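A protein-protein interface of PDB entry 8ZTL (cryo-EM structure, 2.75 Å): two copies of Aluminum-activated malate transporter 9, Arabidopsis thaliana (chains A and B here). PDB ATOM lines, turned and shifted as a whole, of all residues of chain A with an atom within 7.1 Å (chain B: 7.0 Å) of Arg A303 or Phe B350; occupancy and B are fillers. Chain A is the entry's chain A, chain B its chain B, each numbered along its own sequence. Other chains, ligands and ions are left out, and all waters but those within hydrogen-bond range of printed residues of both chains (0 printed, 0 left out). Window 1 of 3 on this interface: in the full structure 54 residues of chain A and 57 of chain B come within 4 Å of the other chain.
The side-chain sulfur (SG) of Cys B348 is in hydrogen-bond range of the backbone carbonyl oxygen (O) of Arg B550 (3.4 Å). The guanidinium group of Arg B550 is in hydrogen-bond range of the backbone carbonyl oxygen of His B347, 2.9 Å away. NH1 of Arg A303 is in hydrogen-bond range of OH of Tyr A299 (2.9 Å).
Of the 18 printed residues of chain A, 3 touch a printed residue of chain B. Hydrophobic or aromatic side chains of chain B that line the printed part of chain A: Phe B350 and Met B353. Among the printed residues, 3 pairs touch across the chains.
Among the printed residues, pairs that only touch across the chains: Arg A303 with Phe B350 (3.7 Å), Met A353 with Met B353 (3.9 Å) and Gly A357 with Arg B550 (3.8 Å).
Met B353 touches its own counterpart, Met A353. Positions printed for both chains: 302, 306, 349, 353 and 356. Of the 3 pairs that touch across the chains among the printed residues, 1 has its exchanged pair printed and touching as well.
Arg A303 touches one residue of chain B. Of the printed residues of chain B, Gly A357 touches Arg B550. Cys B348 touches none of the printed residues of chain A. Phe B350 touches one residue of chain A. Of the printed residues of chain A, Met B353 touches Met A353. The nearest residue of chain B that does not touch Arg A303 is Lys B346 (5.8 Å). The nearest residue of chain A that does not touch Phe B350 is Met A353 (4.4 Å). The nearest printed residue of chain B that does not touch Met A353 is Phe B350 (4.4 Å).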
ATOM      1  N   ASN A 260      -6.716   2.763 -30.584  1.00  0.00           N
ATOM      2  CA  ASN A 260      -7.513   3.250 -29.462  1.00  0.00           C
ATOM      3  C   ASN A 260      -8.810   3.898 -29.935  1.00  0.00           C
ATOM      4  O   ASN A 260      -9.853   3.752 -29.279  1.00  0.00           O
ATOM      5  CB  ASN A 260      -6.700   4.243 -28.631  1.00  0.00           C
ATOM      6  CG  ASN A 260      -5.642   3.564 -27.785  1.00  0.00           C
ATOM      7  OD1 ASN A 260      -5.693   2.357 -27.561  1.00  0.00           O
ATOM      8  ND2 ASN A 260      -4.677   4.339 -27.309  1.00  0.00           N
ATOM      9  N   ASN A 263     -11.149   0.978 -30.651  1.00  0.00           N
ATOM     10  CA  ASN A 263     -11.588   0.332 -29.418  1.00  0.00           C
ATOM     11  C   ASN A 263     -12.675   1.143 -28.725  1.00  0.00           C
ATOM     12  O   ASN A 263     -13.669   0.579 -28.247  1.00  0.00           O
ATOM     13  CB  ASN A 263     -10.400   0.122 -28.481  1.00  0.00           C
ATOM     14  CG  ASN A 263      -9.465  -0.964 -28.960  1.00  0.00           C
ATOM     15  OD1 ASN A 263      -9.805  -1.746 -29.847  1.00  0.00           O
ATOM     16  ND2 ASN A 263      -8.279  -1.024 -28.370  1.00  0.00           N
ATOM     17  N   SER A 267     -16.522  -0.067 -27.900  1.00  0.00           N
ATOM     18  CA  SER A 267     -17.039  -0.078 -26.533  1.00  0.00           C
ATOM     19  C   SER A 267     -18.339   0.709 -26.419  1.00  0.00           C
ATOM     20  O   SER A 267     -19.276   0.273 -25.738  1.00  0.00           O
ATOM     21  CB  SER A 267     -15.997   0.472 -25.563  1.00  0.00           C
ATOM     22  OG  SER A 267     -14.982  -0.482 -25.319  1.00  0.00           O
ATOM     23  N   VAL A 298     -16.345  -4.387 -25.235  1.00  0.00           N
ATOM     24  CA  VAL A 298     -17.285  -3.834 -24.267  1.00  0.00           C
ATOM     25  C   VAL A 298     -16.579  -3.557 -22.947  1.00  0.00           C
ATOM     26  O   VAL A 298     -16.973  -2.665 -22.198  1.00  0.00           O
ATOM     27  CB  VAL A 298     -18.486  -4.770 -24.056  1.00  0.00           C
ATOM     28  CG1 VAL A 298     -19.466  -4.156 -23.066  1.00  0.00           C
ATOM     29  CG2 VAL A 298     -19.170  -5.061 -25.383  1.00  0.00           C
ATOM     30  N   TYR A 299     -15.534  -4.331 -22.665  1.00  0.00           N
ATOM     31  CA  TYR A 299     -14.762  -4.187 -21.437  1.00  0.00           C
ATOM     32  C   TYR A 299     -13.315  -3.807 -21.703  1.00  0.00           C
ATOM     33  O   TYR A 299     -12.795  -2.886 -21.065  1.00  0.00           O
ATOM     34  CB  TYR A 299     -14.819  -5.489 -20.623  1.00  0.00           C
ATOM     35  CG  TYR A 299     -14.319  -5.352 -19.203  1.00  0.00           C
ATOM     36  CD1 TYR A 299     -12.967  -5.469 -18.907  1.00  0.00           C
ATOM     37  CD2 TYR A 299     -15.199  -5.116 -18.157  1.00  0.00           C
ATOM     38  CE1 TYR A 299     -12.508  -5.346 -17.611  1.00  0.00           C
ATOM     39  CE2 TYR A 299     -14.751  -4.993 -16.858  1.00  0.00           C
ATOM     40  CZ  TYR A 299     -13.405  -5.110 -16.589  1.00  0.00           C
ATOM     41  OH  TYR A 299     -12.954  -4.987 -15.295  1.00  0.00           O
ATOM     42  N   LYS A 300     -12.644  -4.499 -22.622  1.00  0.00           N
ATOM     43  CA  LYS A 300     -11.258  -4.177 -22.928  1.00  0.00           C
ATOM     44  C   LYS A 300     -11.117  -2.957 -23.828  1.00  0.00           C
ATOM     45  O   LYS A 300     -10.014  -2.410 -23.926  1.00  0.00           O
ATOM     46  CB  LYS A 300     -10.573  -5.380 -23.581  1.00  0.00           C
ATOM     47  N   GLY A 301     -12.209  -2.472 -24.414  1.00  0.00           N
ATOM     48  CA  GLY A 301     -12.136  -1.353 -25.331  1.00  0.00           C
ATOM     49  C   GLY A 301     -11.649  -0.088 -24.658  1.00  0.00           C
ATOM     50  O   GLY A 301     -10.601   0.449 -25.022  1.00  0.00           O
ATOM     51  N   TYR A 302     -12.404   0.403 -23.676  1.00  0.00           N
ATOM     52  CA  TYR A 302     -11.982   1.602 -22.966  1.00  0.00           C
ATOM     53  C   TYR A 302     -10.775   1.327 -22.079  1.00  0.00           C
ATOM     54  O   TYR A 302      -9.981   2.236 -21.812  1.00  0.00           O
ATOM     55  CB  TYR A 302     -13.143   2.174 -22.147  1.00  0.00           C
ATOM     56  CG  TYR A 302     -13.670   1.261 -21.059  1.00  0.00           C
ATOM     57  CD1 TYR A 302     -13.039   1.176 -19.828  1.00  0.00           C
ATOM     58  CD2 TYR A 302     -14.813   0.501 -21.260  1.00  0.00           C
ATOM     59  CE1 TYR A 302     -13.522   0.350 -18.833  1.00  0.00           C
ATOM     60  CE2 TYR A 302     -15.304  -0.327 -20.271  1.00  0.00           C
ATOM     61  CZ  TYR A 302     -14.654  -0.398 -19.060  1.00  0.00           C
ATOM     62  OH  TYR A 302     -15.138  -1.220 -18.072  1.00  0.00           O
ATOM     63  N   ARG A 303     -10.620   0.083 -21.616  1.00  0.00           N
ATOM     64  CA  ARG A 303      -9.472  -0.257 -20.782  1.00  0.00           C
ATOM     65  C   ARG A 303      -8.163  -0.093 -21.542  1.00  0.00           C
ATOM     66  O   ARG A 303      -7.169   0.387 -20.984  1.00  0.00           O
ATOM     67  CB  ARG A 303      -9.613  -1.684 -20.253  1.00  0.00           C
ATOM     68  CG  ARG A 303     -10.488  -1.797 -19.020  1.00  0.00           C
ATOM     69  CD  ARG A 303      -9.684  -1.552 -17.753  1.00  0.00           C
ATOM     70  NE  ARG A 303     -10.439  -0.803 -16.757  1.00  0.00           N
ATOM     71  CZ  ARG A 303     -11.518  -1.259 -16.136  1.00  0.00           C
ATOM     72  NH1 ARG A 303     -11.997  -2.466 -16.381  1.00  0.00           N
ATOM     73  NH2 ARG A 303     -12.131  -0.485 -15.245  1.00  0.00           N
ATOM     74  N   SER A 304      -8.138  -0.486 -22.818  1.00  0.00           N
ATOM     75  CA  SER A 304      -6.927  -0.320 -23.612  1.00  0.00           C
ATOM     76  C   SER A 304      -6.560   1.152 -23.754  1.00  0.00           C
ATOM     77  O   SER A 304      -5.382   1.517 -23.675  1.00  0.00           O
ATOM     78  CB  SER A 304      -7.111  -0.965 -24.985  1.00  0.00           C
ATOM     79  OG  SER A 304      -7.395  -2.348 -24.862  1.00  0.00           O
ATOM     80  N   ALA A 305      -7.560   2.012 -23.961  1.00  0.00           N
ATOM     81  CA  ALA A 305      -7.292   3.435 -24.137  1.00  0.00           C
ATOM     82  C   ALA A 305      -6.906   4.113 -22.830  1.00  0.00           C
ATOM     83  O   ALA A 305      -6.134   5.078 -22.841  1.00  0.00           O
ATOM     84  CB  ALA A 305      -8.512   4.124 -24.747  1.00  0.00           C
ATOM     85  N   VAL A 306      -7.424   3.631 -21.700  1.00  0.00           N
ATOM     86  CA  VAL A 306      -7.195   4.321 -20.434  1.00  0.00           C
ATOM     87  C   VAL A 306      -5.828   3.990 -19.841  1.00  0.00           C
ATOM     88  O   VAL A 306      -5.207   4.845 -19.200  1.00  0.00           O
ATOM     89  CB  VAL A 306      -8.322   3.987 -19.442  1.00  0.00           C
ATOM     90  CG1 VAL A 306      -7.901   4.334 -18.024  1.00  0.00           C
ATOM     91  CG2 VAL A 306      -9.600   4.721 -19.819  1.00  0.00           C
ATOM     92  N   GLU A 307      -5.335   2.770 -20.038  1.00  0.00           N
ATOM     93  CA  GLU A 307      -4.116   2.303 -19.390  1.00  0.00           C
ATOM     94  C   GLU A 307      -2.888   2.337 -20.295  1.00  0.00           C
ATOM     95  O   GLU A 307      -1.870   1.726 -19.956  1.00  0.00           O
ATOM     96  CB  GLU A 307      -4.325   0.884 -18.856  1.00  0.00           C
ATOM     97  N   SER A 308      -2.951   3.027 -21.433  1.00  0.00           N
ATOM     98  CA  SER A 308      -1.843   3.052 -22.379  1.00  0.00           C
ATOM     99  C   SER A 308      -1.007   4.325 -22.305  1.00  0.00           C
ATOM    100  O   SER A 308      -0.196   4.569 -23.203  1.00  0.00           O
ATOM    101  CB  SER A 308      -2.368   2.865 -23.805  1.00  0.00           C
ATOM    102  OG  SER A 308      -2.765   4.101 -24.369  1.00  0.00           O
ATOM    103  N   ALA A 349     -13.177   8.548 -22.904  1.00  0.00           N
ATOM    104  CA  ALA A 349     -13.414   7.159 -22.506  1.00  0.00           C
ATOM    105  C   ALA A 349     -13.829   7.006 -21.042  1.00  0.00           C
ATOM    106  O   ALA A 349     -14.426   5.978 -20.680  1.00  0.00           O
ATOM    107  CB  ALA A 349     -12.169   6.316 -22.774  1.00  0.00           C
ATOM    108  N   MET A 353     -16.650   4.330 -19.435  1.00  0.00           N
ATOM    109  CA  MET A 353     -16.464   3.472 -18.266  1.00  0.00           C
ATOM    110  C   MET A 353     -17.587   3.680 -17.254  1.00  0.00           C
ATOM    111  O   MET A 353     -18.100   2.716 -16.664  1.00  0.00           O
ATOM    112  CB  MET A 353     -15.108   3.746 -17.623  1.00  0.00           C
ATOM    113  CG  MET A 353     -14.644   2.662 -16.669  1.00  0.00           C
ATOM    114  SD  MET A 353     -13.687   3.316 -15.292  1.00  0.00           S
ATOM    115  CE  MET A 353     -12.475   4.299 -16.165  1.00  0.00           C
ATOM    116  N   HIS A 356     -20.584   1.820 -18.507  1.00  0.00           N
ATOM    117  CA  HIS A 356     -20.492   0.385 -18.265  1.00  0.00           C
ATOM    118  C   HIS A 356     -20.784   0.051 -16.812  1.00  0.00           C
ATOM    119  O   HIS A 356     -21.358  -1.003 -16.523  1.00  0.00           O
ATOM    120  CB  HIS A 356     -19.115  -0.150 -18.646  1.00  0.00           C
ATOM    121  CG  HIS A 356     -19.010  -1.641 -18.559  1.00  0.00           C
ATOM    122  ND1 HIS A 356     -17.835  -2.290 -18.249  1.00  0.00           N
ATOM    123  CD2 HIS A 356     -19.941  -2.610 -18.729  1.00  0.00           C
ATOM    124  CE1 HIS A 356     -18.044  -3.593 -18.239  1.00  0.00           C
ATOM    125  NE2 HIS A 356     -19.313  -3.814 -18.527  1.00  0.00           N
ATOM    126  N   GLY A 357     -20.400   0.932 -15.887  1.00  0.00           N
ATOM    127  CA  GLY A 357     -20.681   0.655 -14.489  1.00  0.00           C
ATOM    128  C   GLY A 357     -22.160   0.592 -14.151  1.00  0.00           C
ATOM    129  O   GLY A 357     -22.528  -0.004 -13.135  1.00  0.00           O
ATOM    130  N   TYR B 302      -8.598   7.261  -4.707  1.00  0.00           N
ATOM    131  CA  TYR B 302      -9.076   6.137  -5.499  1.00  0.00           C
ATOM    132  C   TYR B 302      -8.057   5.695  -6.543  1.00  0.00           C
ATOM    133  O   TYR B 302      -8.115   4.544  -6.993  1.00  0.00           O
ATOM    134  CB  TYR B 302     -10.419   6.471  -6.160  1.00  0.00           C
ATOM    135  CG  TYR B 302     -10.400   7.606  -7.157  1.00  0.00           C
ATOM    136  CD1 TYR B 302      -9.944   7.413  -8.453  1.00  0.00           C
ATOM    137  CD2 TYR B 302     -10.866   8.867  -6.811  1.00  0.00           C
ATOM    138  CE1 TYR B 302      -9.935   8.443  -9.368  1.00  0.00           C
ATOM    139  CE2 TYR B 302     -10.862   9.904  -7.721  1.00  0.00           C
ATOM    140  CZ  TYR B 302     -10.395   9.686  -8.997  1.00  0.00           C
ATOM    141  OH  TYR B 302     -10.388  10.714  -9.909  1.00  0.00           O
ATOM    142  N   VAL B 306      -7.215   1.759  -7.188  1.00  0.00           N
ATOM    143  CA  VAL B 306      -7.587   1.202  -8.485  1.00  0.00           C
ATOM    144  C   VAL B 306      -6.352   0.785  -9.272  1.00  0.00           C
ATOM    145  O   VAL B 306      -6.414  -0.125 -10.107  1.00  0.00           O
ATOM    146  CB  VAL B 306      -8.433   2.202  -9.294  1.00  0.00           C
ATOM    147  CG1 VAL B 306      -8.871   1.578 -10.604  1.00  0.00           C
ATOM    148  CG2 VAL B 306      -9.642   2.650  -8.489  1.00  0.00           C
ATOM    149  N   LEU B 345     -12.996  -3.889  -2.052  1.00  0.00           N
ATOM    150  CA  LEU B 345     -12.914  -2.441  -1.858  1.00  0.00           C
ATOM    151  C   LEU B 345     -12.781  -1.677  -3.179  1.00  0.00           C
ATOM    152  O   LEU B 345     -13.306  -0.562  -3.306  1.00  0.00           O
ATOM    153  CB  LEU B 345     -11.748  -2.104  -0.932  1.00  0.00           C
ATOM    154  CG  LEU B 345     -11.563  -0.621  -0.609  1.00  0.00           C
ATOM    155  CD1 LEU B 345     -12.592  -0.166   0.405  1.00  0.00           C
ATOM    156  CD2 LEU B 345     -10.160  -0.353  -0.106  1.00  0.00           C
ATOM    157  N   LYS B 346     -12.090  -2.248  -4.168  1.00  0.00           N
ATOM    158  CA  LYS B 346     -11.945  -1.569  -5.457  1.00  0.00           C
ATOM    159  C   LYS B 346     -13.286  -1.448  -6.178  1.00  0.00           C
ATOM    160  O   LYS B 346     -13.578  -0.419  -6.825  1.00  0.00           O
ATOM    161  CB  LYS B 346     -10.932  -2.332  -6.309  1.00  0.00           C
ATOM    162  CG  LYS B 346     -10.404  -1.598  -7.518  1.00  0.00           C
ATOM    163  CD  LYS B 346     -10.083  -2.588  -8.624  1.00  0.00           C
ATOM    164  CE  LYS B 346      -9.794  -1.889  -9.936  1.00  0.00           C
ATOM    165  NZ  LYS B 346      -9.101  -2.794 -10.895  1.00  0.00           N
ATOM    166  N   HIS B 347     -14.127  -2.479  -6.056  1.00  0.00           N
ATOM    167  CA  HIS B 347     -15.458  -2.394  -6.644  1.00  0.00           C
ATOM    168  C   HIS B 347     -16.236  -1.210  -6.082  1.00  0.00           C
ATOM    169  O   HIS B 347     -17.049  -0.609  -6.793  1.00  0.00           O
ATOM    170  CB  HIS B 347     -16.227  -3.694  -6.413  1.00  0.00           C
ATOM    171  CG  HIS B 347     -17.420  -3.854  -7.302  1.00  0.00           C
ATOM    172  ND1 HIS B 347     -18.703  -3.964  -6.813  1.00  0.00           N
ATOM    173  CD2 HIS B 347     -17.525  -3.914  -8.650  1.00  0.00           C
ATOM    174  CE1 HIS B 347     -19.547  -4.087  -7.821  1.00  0.00           C
ATOM    175  NE2 HIS B 347     -18.858  -4.061  -8.947  1.00  0.00           N
ATOM    176  N   CYS B 348     -16.001  -0.861  -4.816  1.00  0.00           N
ATOM    177  CA  CYS B 348     -16.625   0.320  -4.229  1.00  0.00           C
ATOM    178  C   CYS B 348     -15.948   1.610  -4.677  1.00  0.00           C
ATOM    179  O   CYS B 348     -16.624   2.630  -4.845  1.00  0.00           O
ATOM    180  CB  CYS B 348     -16.596   0.227  -2.703  1.00  0.00           C
ATOM    181  SG  CYS B 348     -18.047  -0.535  -1.959  1.00  0.00           S
ATOM    182  N   ALA B 349     -14.628   1.589  -4.870  1.00  0.00           N
ATOM    183  CA  ALA B 349     -13.921   2.814  -5.237  1.00  0.00           C
ATOM    184  C   ALA B 349     -14.262   3.290  -6.647  1.00  0.00           C
ATOM    185  O   ALA B 349     -14.070   4.476  -6.959  1.00  0.00           O
ATOM    186  CB  ALA B 349     -12.412   2.610  -5.111  1.00  0.00           C
ATOM    187  N   PHE B 350     -14.798   2.411  -7.495  1.00  0.00           N
ATOM    188  CA  PHE B 350     -15.186   2.879  -8.830  1.00  0.00           C
ATOM    189  C   PHE B 350     -16.326   3.904  -8.771  1.00  0.00           C
ATOM    190  O   PHE B 350     -16.357   4.865  -9.557  1.00  0.00           O
ATOM    191  CB  PHE B 350     -15.586   1.697  -9.711  1.00  0.00           C
ATOM    192  CG  PHE B 350     -14.427   1.006 -10.365  1.00  0.00           C
ATOM    193  CD1 PHE B 350     -13.515   1.721 -11.119  1.00  0.00           C
ATOM    194  CD2 PHE B 350     -14.248  -0.357 -10.226  1.00  0.00           C
ATOM    195  CE1 PHE B 350     -12.446   1.087 -11.721  1.00  0.00           C
ATOM    196  CE2 PHE B 350     -13.181  -0.994 -10.825  1.00  0.00           C
ATOM    197  CZ  PHE B 350     -12.279  -0.271 -11.571  1.00  0.00           C
ATOM    198  N   THR B 351     -17.260   3.739  -7.832  1.00  0.00           N
ATOM    199  CA  THR B 351     -18.330   4.723  -7.682  1.00  0.00           C
ATOM    200  C   THR B 351     -17.792   6.071  -7.216  1.00  0.00           C
ATOM    201  O   THR B 351     -18.287   7.123  -7.637  1.00  0.00           O
ATOM    202  CB  THR B 351     -19.394   4.211  -6.714  1.00  0.00           C
ATOM    203  OG1 THR B 351     -19.972   3.008  -7.234  1.00  0.00           O
ATOM    204  CG2 THR B 351     -20.486   5.251  -6.537  1.00  0.00           C
ATOM    205  N   VAL B 352     -16.790   6.065  -6.337  1.00  0.00           N
ATOM    206  CA  VAL B 352     -16.179   7.323  -5.927  1.00  0.00           C
ATOM    207  C   VAL B 352     -15.486   7.978  -7.112  1.00  0.00           C
ATOM    208  O   VAL B 352     -15.476   9.210  -7.236  1.00  0.00           O
ATOM    209  CB  VAL B 352     -15.217   7.091  -4.747  1.00  0.00           C
ATOM    210  CG1 VAL B 352     -14.730   8.410  -4.189  1.00  0.00           C
ATOM    211  CG2 VAL B 352     -15.903   6.282  -3.667  1.00  0.00           C
ATOM    212  N   MET B 353     -14.910   7.175  -8.007  1.00  0.00           N
ATOM    213  CA  MET B 353     -14.337   7.740  -9.227  1.00  0.00           C
ATOM    214  C   MET B 353     -15.407   8.434 -10.069  1.00  0.00           C
ATOM    215  O   MET B 353     -15.177   9.523 -10.613  1.00  0.00           O
ATOM    216  CB  MET B 353     -13.652   6.645 -10.039  1.00  0.00           C
ATOM    217  CG  MET B 353     -12.491   7.128 -10.882  1.00  0.00           C
ATOM    218  SD  MET B 353     -12.420   6.319 -12.487  1.00  0.00           S
ATOM    219  CE  MET B 353     -12.094   4.631 -11.993  1.00  0.00           C
ATOM    220  N   ALA B 354     -16.590   7.827 -10.175  1.00  0.00           N
ATOM    221  CA  ALA B 354     -17.664   8.468 -10.937  1.00  0.00           C
ATOM    222  C   ALA B 354     -18.157   9.745 -10.253  1.00  0.00           C
ATOM    223  O   ALA B 354     -18.483  10.739 -10.921  1.00  0.00           O
ATOM    224  CB  ALA B 354     -18.818   7.489 -11.141  1.00  0.00           C
ATOM    225  N   LEU B 355     -18.191   9.749  -8.919  1.00  0.00           N
ATOM    226  CA  LEU B 355     -18.587  10.957  -8.200  1.00  0.00           C
ATOM    227  C   LEU B 355     -17.578  12.079  -8.409  1.00  0.00           C
ATOM    228  O   LEU B 355     -17.958  13.249  -8.517  1.00  0.00           O
ATOM    229  CB  LEU B 355     -18.759  10.660  -6.711  1.00  0.00           C
ATOM    230  CG  LEU B 355     -20.002   9.874  -6.294  1.00  0.00           C
ATOM    231  CD1 LEU B 355     -19.801   9.241  -4.931  1.00  0.00           C
ATOM    232  CD2 LEU B 355     -21.221  10.780  -6.289  1.00  0.00           C
ATOM    233  N   HIS B 356     -16.286  11.746  -8.464  1.00  0.00           N
ATOM    234  CA  HIS B 356     -15.290  12.758  -8.801  1.00  0.00           C
ATOM    235  C   HIS B 356     -15.484  13.263 -10.223  1.00  0.00           C
ATOM    236  O   HIS B 356     -15.366  14.465 -10.485  1.00  0.00           O
ATOM    237  CB  HIS B 356     -13.876  12.209  -8.633  1.00  0.00           C
ATOM    238  CG  HIS B 356     -12.806  13.235  -8.849  1.00  0.00           C
ATOM    239  ND1 HIS B 356     -11.666  12.980  -9.578  1.00  0.00           N
ATOM    240  CD2 HIS B 356     -12.713  14.525  -8.447  1.00  0.00           C
ATOM    241  CE1 HIS B 356     -10.911  14.063  -9.606  1.00  0.00           C
ATOM    242  NE2 HIS B 356     -11.524  15.016  -8.927  1.00  0.00           N
ATOM    243  N   LEU B 543     -25.640   8.076  -7.590  1.00  0.00           N
ATOM    244  CA  LEU B 543     -24.327   7.478  -7.402  1.00  0.00           C
ATOM    245  C   LEU B 543     -23.996   7.346  -5.924  1.00  0.00           C
ATOM    246  O   LEU B 543     -23.350   6.372  -5.514  1.00  0.00           O
ATOM    247  CB  LEU B 543     -23.273   8.320  -8.120  1.00  0.00           C
ATOM    248  CG  LEU B 543     -23.138   8.113  -9.629  1.00  0.00           C
ATOM    249  CD1 LEU B 543     -22.269   9.195 -10.238  1.00  0.00           C
ATOM    250  CD2 LEU B 543     -22.569   6.740  -9.931  1.00  0.00           C
ATOM    251  N   ARG B 550     -23.221  -0.741  -2.081  1.00  0.00           N
ATOM    252  CA  ARG B 550     -22.156  -1.712  -2.355  1.00  0.00           C
ATOM    253  C   ARG B 550     -21.304  -2.122  -1.142  1.00  0.00           C
ATOM    254  O   ARG B 550     -20.371  -2.912  -1.315  1.00  0.00           O
ATOM    255  CB  ARG B 550     -21.226  -1.183  -3.453  1.00  0.00           C
ATOM    256  CG  ARG B 550     -21.876  -1.050  -4.817  1.00  0.00           C
ATOM    257  CD  ARG B 550     -20.857  -0.686  -5.886  1.00  0.00           C
ATOM    258  NE  ARG B 550     -21.476  -0.545  -7.200  1.00  0.00           N
ATOM    259  CZ  ARG B 550     -20.808  -0.397  -8.335  1.00  0.00           C
ATOM    260  NH1 ARG B 550     -19.485  -0.360  -8.360  1.00  0.00           N
ATOM    261  NH2 ARG B 550     -21.483  -0.284  -9.475  1.00  0.00           N
